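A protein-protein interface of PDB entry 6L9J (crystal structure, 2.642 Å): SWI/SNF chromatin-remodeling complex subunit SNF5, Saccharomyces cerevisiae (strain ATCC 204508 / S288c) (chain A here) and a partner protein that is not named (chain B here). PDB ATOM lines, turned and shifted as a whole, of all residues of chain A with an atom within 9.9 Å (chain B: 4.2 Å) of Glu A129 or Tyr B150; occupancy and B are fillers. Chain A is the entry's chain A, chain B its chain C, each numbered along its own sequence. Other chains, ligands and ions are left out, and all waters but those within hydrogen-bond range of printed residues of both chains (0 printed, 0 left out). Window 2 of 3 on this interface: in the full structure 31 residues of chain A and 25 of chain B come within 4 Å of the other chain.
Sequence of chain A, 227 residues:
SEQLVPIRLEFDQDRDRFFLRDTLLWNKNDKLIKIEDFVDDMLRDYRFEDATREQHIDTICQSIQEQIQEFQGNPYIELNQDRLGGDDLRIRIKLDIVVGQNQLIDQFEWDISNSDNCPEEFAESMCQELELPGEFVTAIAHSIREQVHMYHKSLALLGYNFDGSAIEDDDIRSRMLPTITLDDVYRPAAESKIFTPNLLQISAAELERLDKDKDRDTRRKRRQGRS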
ATOM      1  N   LEU A 104     -15.079  -5.705  20.179  1.00  0.00           N
ATOM      2  CA  LEU A 104     -14.500  -6.749  19.349  1.00  0.00           C
ATOM      3  C   LEU A 104     -13.094  -6.334  18.959  1.00  0.00           C
ATOM      4  O   LEU A 104     -12.903  -5.256  18.396  1.00  0.00           O
ATOM      5  CB  LEU A 104     -15.360  -7.003  18.112  1.00  0.00           C
ATOM      6  CG  LEU A 104     -14.828  -7.876  16.957  1.00  0.00           C
ATOM      7  CD1 LEU A 104     -14.940  -9.358  17.257  1.00  0.00           C
ATOM      8  CD2 LEU A 104     -15.577  -7.544  15.692  1.00  0.00           C
ATOM      9  N   ASP A 106      -9.778  -7.872  16.748  1.00  0.00           N
ATOM     10  CA  ASP A 106      -9.647  -8.885  15.707  1.00  0.00           C
ATOM     11  C   ASP A 106      -8.602  -8.459  14.689  1.00  0.00           C
ATOM     12  O   ASP A 106      -8.266  -7.282  14.568  1.00  0.00           O
ATOM     13  CB  ASP A 106     -10.983  -9.140  14.998  1.00  0.00           C
ATOM     14  CG  ASP A 106     -11.005 -10.457  14.238  1.00  0.00           C
ATOM     15  OD1 ASP A 106      -9.924 -10.971  13.897  1.00  0.00           O
ATOM     16  OD2 ASP A 106     -12.106 -10.978  13.992  1.00  0.00           O
ATOM     17  N   GLU A 121     -20.204  -9.057   2.604  1.00  0.00           N
ATOM     18  CA  GLU A 121     -20.472 -10.486   2.710  1.00  0.00           C
ATOM     19  C   GLU A 121     -19.676 -11.099   3.852  1.00  0.00           C
ATOM     20  O   GLU A 121     -20.142 -12.028   4.515  1.00  0.00           O
ATOM     21  CB  GLU A 121     -20.144 -11.181   1.396  1.00  0.00           C
ATOM     22  CG  GLU A 121     -20.916 -12.452   1.165  1.00  0.00           C
ATOM     23  CD  GLU A 121     -20.451 -13.195  -0.080  1.00  0.00           C
ATOM     24  OE1 GLU A 121     -19.552 -12.685  -0.775  1.00  0.00           O
ATOM     25  OE2 GLU A 121     -20.974 -14.295  -0.357  1.00  0.00           O
ATOM     26  N   PHE A 122     -18.470 -10.587   4.082  1.00  0.00           N
ATOM     27  CA  PHE A 122     -17.620 -11.060   5.164  1.00  0.00           C
ATOM     28  C   PHE A 122     -18.154 -10.598   6.510  1.00  0.00           C
ATOM     29  O   PHE A 122     -18.452 -11.412   7.388  1.00  0.00           O
ATOM     30  CB  PHE A 122     -16.206 -10.541   4.939  1.00  0.00           C
ATOM     31  CG  PHE A 122     -15.180 -11.210   5.768  1.00  0.00           C
ATOM     32  CD1 PHE A 122     -14.676 -12.437   5.397  1.00  0.00           C
ATOM     33  CD2 PHE A 122     -14.697 -10.604   6.912  1.00  0.00           C
ATOM     34  CE1 PHE A 122     -13.720 -13.051   6.152  1.00  0.00           C
ATOM     35  CE2 PHE A 122     -13.737 -11.212   7.677  1.00  0.00           C
ATOM     36  CZ  PHE A 122     -13.247 -12.435   7.300  1.00  0.00           C
ATOM     37  N   ALA A 123     -18.307  -9.286   6.672  1.00  0.00           N
ATOM     38  CA  ALA A 123     -18.877  -8.737   7.887  1.00  0.00           C
ATOM     39  C   ALA A 123     -20.152  -9.456   8.290  1.00  0.00           C
ATOM     40  O   ALA A 123     -20.427  -9.618   9.482  1.00  0.00           O
ATOM     41  CB  ALA A 123     -19.144  -7.247   7.706  1.00  0.00           C
ATOM     42  N   GLU A 124     -20.938  -9.902   7.331  1.00  0.00           N
ATOM     43  CA  GLU A 124     -22.203 -10.507   7.703  1.00  0.00           C
ATOM     44  C   GLU A 124     -22.050 -11.954   8.142  1.00  0.00           C
ATOM     45  O   GLU A 124     -22.908 -12.451   8.874  1.00  0.00           O
ATOM     46  CB  GLU A 124     -23.204 -10.409   6.557  1.00  0.00           C
ATOM     47  CG  GLU A 124     -24.546 -10.994   6.894  1.00  0.00           C
ATOM     48  CD  GLU A 124     -25.392 -10.082   7.756  1.00  0.00           C
ATOM     49  OE1 GLU A 124     -25.564  -8.902   7.386  1.00  0.00           O
ATOM     50  OE2 GLU A 124     -25.897 -10.550   8.801  1.00  0.00           O
ATOM     51  N   SER A 125     -20.985 -12.643   7.733  1.00  0.00           N
ATOM     52  CA  SER A 125     -20.793 -13.975   8.282  1.00  0.00           C
ATOM     53  C   SER A 125     -20.033 -13.931   9.607  1.00  0.00           C
ATOM     54  O   SER A 125     -20.311 -14.733  10.500  1.00  0.00           O
ATOM     55  CB  SER A 125     -20.084 -14.879   7.277  1.00  0.00           C
ATOM     56  OG  SER A 125     -18.742 -14.506   7.109  1.00  0.00           O
ATOM     57  N   MET A 126     -19.078 -13.008   9.749  1.00  0.00           N
ATOM     58  CA  MET A 126     -18.537 -12.667  11.054  1.00  0.00           C
ATOM     59  C   MET A 126     -19.664 -12.534  12.073  1.00  0.00           C
ATOM     60  O   MET A 126     -19.701 -13.263  13.060  1.00  0.00           O
ATOM     61  CB  MET A 126     -17.703 -11.380  10.971  1.00  0.00           C
ATOM     62  CG  MET A 126     -16.220 -11.617  10.783  1.00  0.00           C
ATOM     63  SD  MET A 126     -15.167 -10.169  10.873  1.00  0.00           S
ATOM     64  CE  MET A 126     -15.217  -9.893  12.633  1.00  0.00           C
ATOM     65  N   CYS A 127     -20.622 -11.644  11.832  1.00  0.00           N
ATOM     66  CA  CYS A 127     -21.671 -11.456  12.826  1.00  0.00           C
ATOM     67  C   CYS A 127     -22.556 -12.668  12.986  1.00  0.00           C
ATOM     68  O   CYS A 127     -23.333 -12.722  13.939  1.00  0.00           O
ATOM     69  CB  CYS A 127     -22.554 -10.271  12.480  1.00  0.00           C
ATOM     70  SG  CYS A 127     -21.656  -8.793  12.373  1.00  0.00           S
ATOM     71  N   GLN A 128     -22.498 -13.612  12.062  1.00  0.00           N
ATOM     72  CA  GLN A 128     -23.275 -14.832  12.207  1.00  0.00           C
ATOM     73  C   GLN A 128     -22.544 -15.840  13.076  1.00  0.00           C
ATOM     74  O   GLN A 128     -23.166 -16.518  13.892  1.00  0.00           O
ATOM     75  CB  GLN A 128     -23.562 -15.438  10.829  1.00  0.00           C
ATOM     76  CG  GLN A 128     -24.561 -14.664   9.986  1.00  0.00           C
ATOM     77  CD  GLN A 128     -25.947 -14.642  10.595  1.00  0.00           C
ATOM     78  OE1 GLN A 128     -26.115 -14.814  11.803  1.00  0.00           O
ATOM     79  NE2 GLN A 128     -26.951 -14.431   9.758  1.00  0.00           N
ATOM     80  N   GLU A 129     -21.223 -15.929  12.914  1.00  0.00           N
ATOM     81  CA  GLU A 129     -20.424 -16.978  13.532  1.00  0.00           C
ATOM     82  C   GLU A 129     -20.078 -16.644  14.974  1.00  0.00           C
ATOM     83  O   GLU A 129     -20.196 -17.500  15.852  1.00  0.00           O
ATOM     84  CB  GLU A 129     -19.146 -17.206  12.722  1.00  0.00           C
ATOM     85  CG  GLU A 129     -19.380 -17.482  11.249  1.00  0.00           C
ATOM     86  CD  GLU A 129     -18.192 -18.126  10.561  1.00  0.00           C
ATOM     87  OE1 GLU A 129     -17.125 -17.495  10.442  1.00  0.00           O
ATOM     88  OE2 GLU A 129     -18.334 -19.281  10.124  1.00  0.00           O
ATOM     89  N   LEU A 130     -19.630 -15.415  15.222  1.00  0.00           N
ATOM     90  CA  LEU A 130     -19.488 -14.849  16.553  1.00  0.00           C
ATOM     91  C   LEU A 130     -20.828 -14.509  17.186  1.00  0.00           C
ATOM     92  O   LEU A 130     -20.868 -14.141  18.363  1.00  0.00           O
ATOM     93  CB  LEU A 130     -18.612 -13.604  16.477  1.00  0.00           C
ATOM     94  CG  LEU A 130     -17.377 -13.891  15.637  1.00  0.00           C
ATOM     95  CD1 LEU A 130     -16.353 -12.803  15.714  1.00  0.00           C
ATOM     96  CD2 LEU A 130     -16.784 -15.210  16.045  1.00  0.00           C
ATOM     97  N   GLU A 131     -21.921 -14.697  16.457  1.00  0.00           N
ATOM     98  CA  GLU A 131     -23.220 -14.136  16.808  1.00  0.00           C
ATOM     99  C   GLU A 131     -23.056 -12.780  17.475  1.00  0.00           C
ATOM    100  O   GLU A 131     -23.360 -12.618  18.660  1.00  0.00           O
ATOM    101  CB  GLU A 131     -24.035 -15.078  17.710  1.00  0.00           C
ATOM    102  CG  GLU A 131     -23.287 -15.905  18.713  1.00  0.00           C
ATOM    103  CD  GLU A 131     -24.045 -17.193  19.019  1.00  0.00           C
ATOM    104  OE1 GLU A 131     -24.307 -17.958  18.073  1.00  0.00           O
ATOM    105  OE2 GLU A 131     -24.397 -17.442  20.187  1.00  0.00           O
ATOM    106  N   LEU A 132     -22.589 -11.808  16.713  1.00  0.00           N
ATOM    107  CA  LEU A 132     -22.485 -10.457  17.190  1.00  0.00           C
ATOM    108  C   LEU A 132     -23.850  -9.782  17.148  1.00  0.00           C
ATOM    109  O   LEU A 132     -24.760 -10.247  16.472  1.00  0.00           O
ATOM    110  CB  LEU A 132     -21.464  -9.700  16.351  1.00  0.00           C
ATOM    111  CG  LEU A 132     -20.068 -10.329  16.305  1.00  0.00           C
ATOM    112  CD1 LEU A 132     -19.124  -9.545  15.445  1.00  0.00           C
ATOM    113  CD2 LEU A 132     -19.470 -10.464  17.706  1.00  0.00           C
ATOM    114  N   PRO A 133     -24.041  -8.722  17.917  1.00  0.00           N
ATOM    115  CA  PRO A 133     -25.214  -7.880  17.696  1.00  0.00           C
ATOM    116  C   PRO A 133     -25.182  -7.311  16.285  1.00  0.00           C
ATOM    117  O   PRO A 133     -24.118  -7.006  15.743  1.00  0.00           O
ATOM    118  CB  PRO A 133     -25.069  -6.793  18.761  1.00  0.00           C
ATOM    119  CG  PRO A 133     -24.159  -7.379  19.779  1.00  0.00           C
ATOM    120  CD  PRO A 133     -23.212  -8.235  19.024  1.00  0.00           C
ATOM    121  N   ILE A 140     -17.988  -3.459  10.908  1.00  0.00           N
ATOM    122  CA  ILE A 140     -16.923  -4.273  10.327  1.00  0.00           C
ATOM    123  C   ILE A 140     -16.725  -3.945   8.851  1.00  0.00           C
ATOM    124  O   ILE A 140     -15.593  -3.983   8.350  1.00  0.00           O
ATOM    125  CB  ILE A 140     -17.198  -5.777  10.509  1.00  0.00           C
ATOM    126  CG1 ILE A 140     -17.489  -6.108  11.967  1.00  0.00           C
ATOM    127  CG2 ILE A 140     -16.019  -6.587  10.030  1.00  0.00           C
ATOM    128  CD1 ILE A 140     -17.896  -7.521  12.186  1.00  0.00           C
ATOM    129  N   PRO A 197     -10.478 -13.458  16.723  1.00  0.00           N
ATOM    130  CA  PRO A 197     -11.338 -12.478  17.387  1.00  0.00           C
ATOM    131  C   PRO A 197     -11.492 -12.691  18.890  1.00  0.00           C
ATOM    132  O   PRO A 197     -11.444 -13.808  19.412  1.00  0.00           O
ATOM    133  CB  PRO A 197     -12.675 -12.692  16.663  1.00  0.00           C
ATOM    134  CG  PRO A 197     -12.676 -14.116  16.397  1.00  0.00           C
ATOM    135  CD  PRO A 197     -11.268 -14.520  16.105  1.00  0.00           C
ATOM    136  N   LEU A 199     -14.076 -10.962  22.007  1.00  0.00           N
ATOM    137  CA  LEU A 199     -15.273 -10.173  22.282  1.00  0.00           C
ATOM    138  C   LEU A 199     -15.398 -10.002  23.798  1.00  0.00           C
ATOM    139  O   LEU A 199     -15.829 -10.923  24.501  1.00  0.00           O
ATOM    140  CB  LEU A 199     -16.505 -10.865  21.697  1.00  0.00           C
ATOM    141  CG  LEU A 199     -17.769 -10.092  21.288  1.00  0.00           C
ATOM    142  CD1 LEU A 199     -18.939 -10.341  22.209  1.00  0.00           C
ATOM    143  CD2 LEU A 199     -17.512  -8.620  21.144  1.00  0.00           C
ATOM    144  N   GLU B 149     -20.755 -30.305  14.693  1.00  0.00           N
ATOM    145  CA  GLU B 149     -20.401 -28.992  15.189  1.00  0.00           C
ATOM    146  C   GLU B 149     -19.904 -28.136  14.039  1.00  0.00           C
ATOM    147  O   GLU B 149     -18.952 -28.506  13.345  1.00  0.00           O
ATOM    148  CB  GLU B 149     -19.335 -29.123  16.282  1.00  0.00           C
ATOM    149  CG  GLU B 149     -18.406 -27.954  16.443  1.00  0.00           C
ATOM    150  CD  GLU B 149     -17.378 -28.198  17.530  1.00  0.00           C
ATOM    151  OE1 GLU B 149     -17.633 -29.047  18.413  1.00  0.00           O
ATOM    152  OE2 GLU B 149     -16.313 -27.546  17.493  1.00  0.00           O
ATOM    153  N   TYR B 150     -20.537 -26.983  13.866  1.00  0.00           N
ATOM    154  CA  TYR B 150     -20.247 -26.083  12.761  1.00  0.00           C
ATOM    155  C   TYR B 150     -18.781 -25.674  12.747  1.00  0.00           C
ATOM    156  O   TYR B 150     -18.289 -25.080  13.703  1.00  0.00           O
ATOM    157  CB  TYR B 150     -21.162 -24.860  12.876  1.00  0.00           C
ATOM    158  CG  TYR B 150     -20.885 -23.763  11.894  1.00  0.00           C
ATOM    159  CD1 TYR B 150     -21.557 -23.697  10.672  1.00  0.00           C
ATOM    160  CD2 TYR B 150     -19.959 -22.781  12.178  1.00  0.00           C
ATOM    161  CE1 TYR B 150     -21.305 -22.683   9.770  1.00  0.00           C
ATOM    162  CE2 TYR B 150     -19.697 -21.770  11.273  1.00  0.00           C
ATOM    163  CZ  TYR B 150     -20.369 -21.727  10.078  1.00  0.00           C
ATOM    164  OH  TYR B 150     -20.080 -20.714   9.207  1.00  0.00           O
ATOM    165  N   PHE B 151     -18.076 -26.003  11.671  1.00  0.00           N
ATOM    166  CA  PHE B 151     -16.754 -25.452  11.413  1.00  0.00           C
ATOM    167  C   PHE B 151     -16.913 -24.099  10.755  1.00  0.00           C
ATOM    168  O   PHE B 151     -17.796 -23.914   9.918  1.00  0.00           O
ATOM    169  CB  PHE B 151     -15.945 -26.381  10.515  1.00  0.00           C
ATOM    170  CG  PHE B 151     -14.623 -25.815  10.070  1.00  0.00           C
ATOM    171  CD1 PHE B 151     -13.444 -26.213  10.676  1.00  0.00           C
ATOM    172  CD2 PHE B 151     -14.551 -24.921   9.017  1.00  0.00           C
ATOM    173  CE1 PHE B 151     -12.236 -25.710  10.262  1.00  0.00           C
ATOM    174  CE2 PHE B 151     -13.339 -24.407   8.609  1.00  0.00           C
ATOM    175  CZ  PHE B 151     -12.187 -24.802   9.222  1.00  0.00           C
ATOM    176  N   SER B 152     -16.044 -23.151  11.110  1.00  0.00           N
ATOM    177  CA  SER B 152     -16.303 -21.754  10.808  1.00  0.00           C
ATOM    178  C   SER B 152     -15.118 -21.110  10.103  1.00  0.00           C
ATOM    179  O   SER B 152     -13.989 -21.596  10.168  1.00  0.00           O
ATOM    180  CB  SER B 152     -16.637 -20.978  12.075  1.00  0.00           C
ATOM    181  OG  SER B 152     -15.466 -20.467  12.674  1.00  0.00           O
ATOM    182  N   VAL B 153     -15.404 -19.995   9.417  1.00  0.00           N
ATOM    183  CA  VAL B 153     -14.367 -19.237   8.725  1.00  0.00           C
ATOM    184  C   VAL B 153     -13.377 -18.657   9.724  1.00  0.00           C
ATOM    185  O   VAL B 153     -12.177 -18.563   9.450  1.00  0.00           O
ATOM    186  CB  VAL B 153     -15.001 -18.126   7.855  1.00  0.00           C
ATOM    187  CG1 VAL B 153     -13.956 -17.409   7.013  1.00  0.00           C
ATOM    188  CG2 VAL B 153     -16.102 -18.685   6.977  1.00  0.00           C
ATOM    189  N   THR B 154     -13.863 -18.244  10.894  1.00  0.00           N
ATOM    190  CA  THR B 154     -12.956 -17.715  11.906  1.00  0.00           C
ATOM    191  C   THR B 154     -11.941 -18.775  12.332  1.00  0.00           C
ATOM    192  O   THR B 154     -10.732 -18.519  12.341  1.00  0.00           O
ATOM    193  CB  THR B 154     -13.723 -17.176  13.118  1.00  0.00           C
ATOM    194  OG1 THR B 154     -15.043 -16.792  12.743  1.00  0.00           O
ATOM    195  CG2 THR B 154     -13.053 -15.935  13.608  1.00  0.00           C
ATOM    196  N   HIS B 171     -14.476 -21.847   1.957  1.00  0.00           N
ATOM    197  CA  HIS B 171     -15.451 -22.354   2.919  1.00  0.00           C
ATOM    198  C   HIS B 171     -16.836 -22.514   2.293  1.00  0.00           C
ATOM    199  O   HIS B 171     -17.535 -23.497   2.559  1.00  0.00           O
ATOM    200  CB  HIS B 171     -15.490 -21.413   4.135  1.00  0.00           C
ATOM    201  CG  HIS B 171     -16.384 -21.876   5.240  1.00  0.00           C
ATOM    202  ND1 HIS B 171     -17.724 -21.568   5.289  1.00  0.00           N
ATOM    203  CD2 HIS B 171     -16.131 -22.623   6.337  1.00  0.00           C
ATOM    204  CE1 HIS B 171     -18.261 -22.116   6.360  1.00  0.00           C
ATOM    205  NE2 HIS B 171     -17.315 -22.758   7.016  1.00  0.00           N
ATOM    206  N   ASN B 181     -19.733 -29.122   7.002  1.00  0.00           N
ATOM    207  CA  ASN B 181     -20.895 -28.695   7.765  1.00  0.00           C
ATOM    208  C   ASN B 181     -22.179 -29.346   7.331  1.00  0.00           C
ATOM    209  O   ASN B 181     -23.261 -28.811   7.580  1.00  0.00           O
ATOM    210  CB  ASN B 181     -21.019 -27.180   7.726  1.00  0.00           C
ATOM    211  CG  ASN B 181     -20.124 -26.538   8.743  1.00  0.00           C
ATOM    212  OD1 ASN B 181     -20.065 -27.012   9.859  1.00  0.00           O
ATOM    213  ND2 ASN B 181     -19.389 -25.502   8.359  1.00  0.00           N
ATOM    214  N   VAL B 184     -24.503 -30.453  10.654  1.00  0.00           N
ATOM    215  CA  VAL B 184     -24.369 -29.658  11.868  1.00  0.00           C
ATOM    216  C   VAL B 184     -25.589 -29.724  12.773  1.00  0.00           C
ATOM    217  O   VAL B 184     -25.471 -29.498  13.980  1.00  0.00           O
ATOM    218  CB  VAL B 184     -24.029 -28.207  11.511  1.00  0.00           C
ATOM    219  CG1 VAL B 184     -24.297 -27.306  12.683  1.00  0.00           C
ATOM    220  CG2 VAL B 184     -22.582 -28.115  11.108  1.00  0.00           C
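The side-chain carboxylate (OE2) of Glu A129 sits at hydrogen-bond distance from the side-chain hydroxyl (OH) of Tyr B150, 2.4 Å away.
OE2 of Glu A129 is in hydrogen-bond range of N of Val B153 (3.1 Å).
OG1 of Thr B154 sits at hydrogen-bond distance from OE1 of Glu A129, 3.2 Å away.
The side-chain hydroxyl (OG) of Ser B152 lies close to the backbone NH (N) of Thr B154, 3.3 Å away.
Glu A129 touches Ser B152.
Pro A197 touches Thr B154 (CG to CG2, 3.4 Å).
Of the printed residues of chain B, Glu A129 touches Tyr B150 (2.4 Å), Ser B152 (3.1 Å), Val B153 (3.1 Å) and Thr B154 (3.2 Å).
No residue of chain A comes within 4 Å of Glu B149.
Of chain A, only Glu A129 comes within 4 Å of Ser B152.
Of the printed residues of chain A, Thr B154 touches Glu A129 (3.2 Å) and Pro A197 (3.4 Å).
Of the printed residues of chain B, Pro A197 touches Thr B154.
The nearest residue of chain A that does not touch Tyr B150 is Ser A125 (6.1 Å).
Hydrophobic or aromatic side chains of chain B that line the printed part of chain A: Tyr B150 and Val B153.
Printed residues of chain A that touch a printed residue of chain B: Glu A129 and Pro A197.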
